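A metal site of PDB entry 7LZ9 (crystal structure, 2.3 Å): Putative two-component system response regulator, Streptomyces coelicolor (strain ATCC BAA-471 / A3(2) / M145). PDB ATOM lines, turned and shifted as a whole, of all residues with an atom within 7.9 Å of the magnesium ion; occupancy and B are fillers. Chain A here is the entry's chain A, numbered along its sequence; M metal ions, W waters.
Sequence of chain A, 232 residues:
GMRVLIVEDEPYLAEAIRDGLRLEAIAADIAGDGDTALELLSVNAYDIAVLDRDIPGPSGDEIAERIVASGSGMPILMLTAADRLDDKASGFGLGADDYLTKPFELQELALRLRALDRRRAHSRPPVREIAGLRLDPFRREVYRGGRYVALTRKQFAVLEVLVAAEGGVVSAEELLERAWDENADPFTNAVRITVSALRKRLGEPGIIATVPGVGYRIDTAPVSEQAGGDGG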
ATOM      1  N   VAL A   7       1.239 -20.550 -18.732  1.00  0.00           N
ATOM      2  CA  VAL A   7       0.087 -21.268 -18.228  1.00  0.00           C
ATOM      3  C   VAL A   7      -1.130 -20.378 -18.416  1.00  0.00           C
ATOM      4  O   VAL A   7      -1.262 -19.331 -17.755  1.00  0.00           O
ATOM      5  CB  VAL A   7       0.255 -21.667 -16.755  1.00  0.00           C
ATOM      6  CG1 VAL A   7      -0.880 -22.557 -16.313  1.00  0.00           C
ATOM      7  CG2 VAL A   7       1.580 -22.381 -16.568  1.00  0.00           C
ATOM      8  N   GLU A   8      -2.018 -20.777 -19.326  1.00  0.00           N
ATOM      9  CA  GLU A   8      -3.208 -19.998 -19.641  1.00  0.00           C
ATOM     10  C   GLU A   8      -4.235 -20.938 -20.256  1.00  0.00           C
ATOM     11  O   GLU A   8      -3.878 -21.737 -21.128  1.00  0.00           O
ATOM     12  CB  GLU A   8      -2.881 -18.841 -20.592  1.00  0.00           C
ATOM     13  CG  GLU A   8      -4.079 -18.243 -21.299  1.00  0.00           C
ATOM     14  CD  GLU A   8      -4.972 -17.439 -20.368  1.00  0.00           C
ATOM     15  OE1 GLU A   8      -4.450 -16.544 -19.656  1.00  0.00           O
ATOM     16  OE2 GLU A   8      -6.195 -17.696 -20.345  1.00  0.00           O
ATOM     17  N   ASP A   9      -5.486 -20.849 -19.812  1.00  0.00           N
ATOM     18  CA  ASP A   9      -6.494 -21.832 -20.198  1.00  0.00           C
ATOM     19  C   ASP A   9      -7.439 -21.362 -21.284  1.00  0.00           C
ATOM     20  O   ASP A   9      -8.098 -22.213 -21.908  1.00  0.00           O
ATOM     21  CB  ASP A   9      -7.324 -22.245 -18.968  1.00  0.00           C
ATOM     22  CG  ASP A   9      -8.044 -21.075 -18.331  1.00  0.00           C
ATOM     23  OD1 ASP A   9      -7.420 -19.993 -18.183  1.00  0.00           O
ATOM     24  OD2 ASP A   9      -9.219 -21.229 -17.958  1.00  0.00           O
ATOM     25  N   GLU A  10      -7.562 -20.061 -21.519  1.00  0.00           N
ATOM     26  CA  GLU A  10      -8.455 -19.572 -22.554  1.00  0.00           C
ATOM     27  C   GLU A  10      -8.094 -20.210 -23.901  1.00  0.00           C
ATOM     28  O   GLU A  10      -6.918 -20.312 -24.238  1.00  0.00           O
ATOM     29  CB  GLU A  10      -8.387 -18.052 -22.666  1.00  0.00           C
ATOM     30  CG  GLU A  10      -9.356 -17.462 -23.685  1.00  0.00           C
ATOM     31  CD  GLU A  10      -9.279 -15.949 -23.778  1.00  0.00           C
ATOM     32  OE1 GLU A  10      -9.424 -15.411 -24.901  1.00  0.00           O
ATOM     33  OE2 GLU A  10      -9.076 -15.305 -22.735  1.00  0.00           O
ATOM     34  N   LEU A  13      -5.243 -19.104 -26.641  1.00  0.00           N
ATOM     35  CA  LEU A  13      -4.476 -17.958 -26.159  1.00  0.00           C
ATOM     36  C   LEU A  13      -3.058 -18.357 -25.774  1.00  0.00           C
ATOM     37  O   LEU A  13      -2.096 -17.666 -26.143  1.00  0.00           O
ATOM     38  CB  LEU A  13      -5.185 -17.305 -24.969  1.00  0.00           C
ATOM     39  CG  LEU A  13      -4.510 -16.024 -24.472  1.00  0.00           C
ATOM     40  CD1 LEU A  13      -4.296 -15.054 -25.615  1.00  0.00           C
ATOM     41  CD2 LEU A  13      -5.310 -15.378 -23.353  1.00  0.00           C
ATOM     42  N   GLY A  32      -2.403 -25.700 -20.090  1.00  0.00           N
ATOM     43  CA  GLY A  32      -3.728 -25.138 -19.935  1.00  0.00           C
ATOM     44  C   GLY A  32      -4.288 -25.272 -18.537  1.00  0.00           C
ATOM     45  O   GLY A  32      -5.344 -24.712 -18.228  1.00  0.00           O
ATOM     46  N   ASP A  52      -1.457 -17.470 -15.734  1.00  0.00           N
ATOM     47  CA  ASP A  52      -2.828 -17.005 -15.551  1.00  0.00           C
ATOM     48  C   ASP A  52      -3.316 -17.403 -14.155  1.00  0.00           C
ATOM     49  O   ASP A  52      -3.047 -18.504 -13.680  1.00  0.00           O
ATOM     50  CB  ASP A  52      -3.742 -17.604 -16.619  1.00  0.00           C
ATOM     51  CG  ASP A  52      -5.141 -17.019 -16.599  1.00  0.00           C
ATOM     52  OD1 ASP A  52      -5.288 -15.843 -16.204  1.00  0.00           O
ATOM     53  OD2 ASP A  52      -6.089 -17.737 -16.982  1.00  0.00           O
ATOM     54  N   ARG A  53      -4.035 -16.495 -13.495  1.00  0.00           N
ATOM     55  CA  ARG A  53      -4.418 -16.735 -12.106  1.00  0.00           C
ATOM     56  C   ARG A  53      -5.535 -17.762 -12.010  1.00  0.00           C
ATOM     57  O   ARG A  53      -5.445 -18.723 -11.231  1.00  0.00           O
ATOM     58  CB  ARG A  53      -4.813 -15.419 -11.443  1.00  0.00           C
ATOM     59  CG  ARG A  53      -3.725 -14.371 -11.494  1.00  0.00           C
ATOM     60  CD  ARG A  53      -3.697 -13.514 -10.240  1.00  0.00           C
ATOM     61  NE  ARG A  53      -4.951 -13.596  -9.494  1.00  0.00           N
ATOM     62  CZ  ARG A  53      -5.172 -12.992  -8.336  1.00  0.00           C
ATOM     63  NH1 ARG A  53      -6.346 -13.103  -7.729  1.00  0.00           N
ATOM     64  NH2 ARG A  53      -4.215 -12.254  -7.788  1.00  0.00           N
ATOM     65  N   ASP A  54      -6.603 -17.592 -12.798  1.00  0.00           N
ATOM     66  CA  ASP A  54      -7.751 -18.497 -12.771  1.00  0.00           C
ATOM     67  C   ASP A  54      -7.576 -19.535 -13.877  1.00  0.00           C
ATOM     68  O   ASP A  54      -7.819 -19.251 -15.055  1.00  0.00           O
ATOM     69  CB  ASP A  54      -9.059 -17.733 -12.920  1.00  0.00           C
ATOM     70  CG  ASP A  54     -10.279 -18.608 -12.658  1.00  0.00           C
ATOM     71  OD1 ASP A  54     -11.413 -18.097 -12.758  1.00  0.00           O
ATOM     72  OD2 ASP A  54     -10.102 -19.806 -12.334  1.00  0.00           O
ATOM     73  N   ILE A  55      -7.168 -20.732 -13.495  1.00  0.00           N
ATOM     74  CA  ILE A  55      -7.001 -21.859 -14.419  1.00  0.00           C
ATOM     75  C   ILE A  55      -7.558 -23.111 -13.766  1.00  0.00           C
ATOM     76  O   ILE A  55      -7.653 -23.206 -12.532  1.00  0.00           O
ATOM     77  CB  ILE A  55      -5.518 -22.077 -14.792  1.00  0.00           C
ATOM     78  CG1 ILE A  55      -4.677 -22.200 -13.522  1.00  0.00           C
ATOM     79  CG2 ILE A  55      -5.011 -20.929 -15.660  1.00  0.00           C
ATOM     80  CD1 ILE A  55      -3.354 -22.859 -13.738  1.00  0.00           C
ATOM     81  N   PRO A  56      -7.940 -24.102 -14.571  1.00  0.00           N
ATOM     82  CA  PRO A  56      -8.339 -25.390 -14.012  1.00  0.00           C
ATOM     83  C   PRO A  56      -7.189 -26.033 -13.238  1.00  0.00           C
ATOM     84  O   PRO A  56      -6.010 -25.763 -13.481  1.00  0.00           O
ATOM     85  CB  PRO A  56      -8.719 -26.235 -15.244  1.00  0.00           C
ATOM     86  CG  PRO A  56      -8.306 -25.426 -16.434  1.00  0.00           C
ATOM     87  CD  PRO A  56      -8.285 -23.999 -16.001  1.00  0.00           C
ATOM     88  N   LEU A  79      -0.839 -13.167 -15.052  1.00  0.00           N
ATOM     89  CA  LEU A  79      -1.805 -12.605 -15.984  1.00  0.00           C
ATOM     90  C   LEU A  79      -3.151 -12.501 -15.281  1.00  0.00           C
ATOM     91  O   LEU A  79      -3.613 -13.461 -14.656  1.00  0.00           O
ATOM     92  CB  LEU A  79      -1.924 -13.470 -17.236  1.00  0.00           C
ATOM     93  CG  LEU A  79      -0.626 -13.766 -17.981  1.00  0.00           C
ATOM     94  CD1 LEU A  79      -0.902 -14.591 -19.221  1.00  0.00           C
ATOM     95  CD2 LEU A  79       0.093 -12.472 -18.338  1.00  0.00           C
ATOM     96  N   ALA A  81      -7.340 -10.752 -15.276  1.00  0.00           N
ATOM     97  CA  ALA A  81      -8.445 -10.147 -16.016  1.00  0.00           C
ATOM     98  C   ALA A  81      -8.664  -8.706 -15.586  1.00  0.00           C
ATOM     99  O   ALA A  81      -8.908  -7.839 -16.436  1.00  0.00           O
ATOM    100  CB  ALA A  81      -9.716 -10.973 -15.816  1.00  0.00           C
ATOM    101  N   LYS A 102      -4.924  -8.669 -19.057  1.00  0.00           N
ATOM    102  CA  LYS A 102      -5.352  -9.108 -20.377  1.00  0.00           C
ATOM    103  C   LYS A 102      -6.519  -8.263 -20.879  1.00  0.00           C
ATOM    104  O   LYS A 102      -7.404  -7.904 -20.085  1.00  0.00           O
ATOM    105  CB  LYS A 102      -5.766 -10.581 -20.358  1.00  0.00           C
ATOM    106  CG  LYS A 102      -4.609 -11.546 -20.208  1.00  0.00           C
ATOM    107  CD  LYS A 102      -5.099 -12.984 -20.131  1.00  0.00           C
ATOM    108  CE  LYS A 102      -5.664 -13.297 -18.768  1.00  0.00           C
ATOM    109  NZ  LYS A 102      -5.956 -14.744 -18.617  1.00  0.00           N
HETATM  110 MG    MG M   1      -8.096 -18.426 -16.917  1.00  0.00          MG
HETATM  111  O   HOH W   1      -8.091 -17.632 -18.874  1.00  0.00           O
HETATM  112  O   HOH W   2      -8.350 -16.379 -16.281  1.00  0.00           O
HETATM  113  O   HOH W   3     -10.028 -19.179 -16.951  1.00  0.00           O
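The backbone carbonyl oxygen of Val 7 is in hydrogen-bond range of the backbone NH of Asp 52. The side-chain amino group (NZ) of Lys 102 is in salt-bridge range of the side-chain carboxylate (OE1) of Glu 8 (2.6 Å). The side-chain carboxylate (OD1) of Asp 52 lies within salt-bridge range of the side-chain amino group (NZ) of Lys 102 (2.7 Å). The backbone NH (N) of Glu 10 lies within hydrogen-bond range of the side-chain carboxylate (OE2) of Glu 8.
Merely in contact with the magnesium ion: Glu 8. Four residues have an atom within 4 Å of the magnesium ion: Glu 8, Asp 9, Asp 52 and Asp 54.
The magnesium ion is bound by the backbone carbonyl oxygen (O) of Asp 54, water W3, water W1, the side-chain carboxylate (OD2) of Asp 52, the side-chain carboxylate (OD1) of Asp 9 and water W2.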
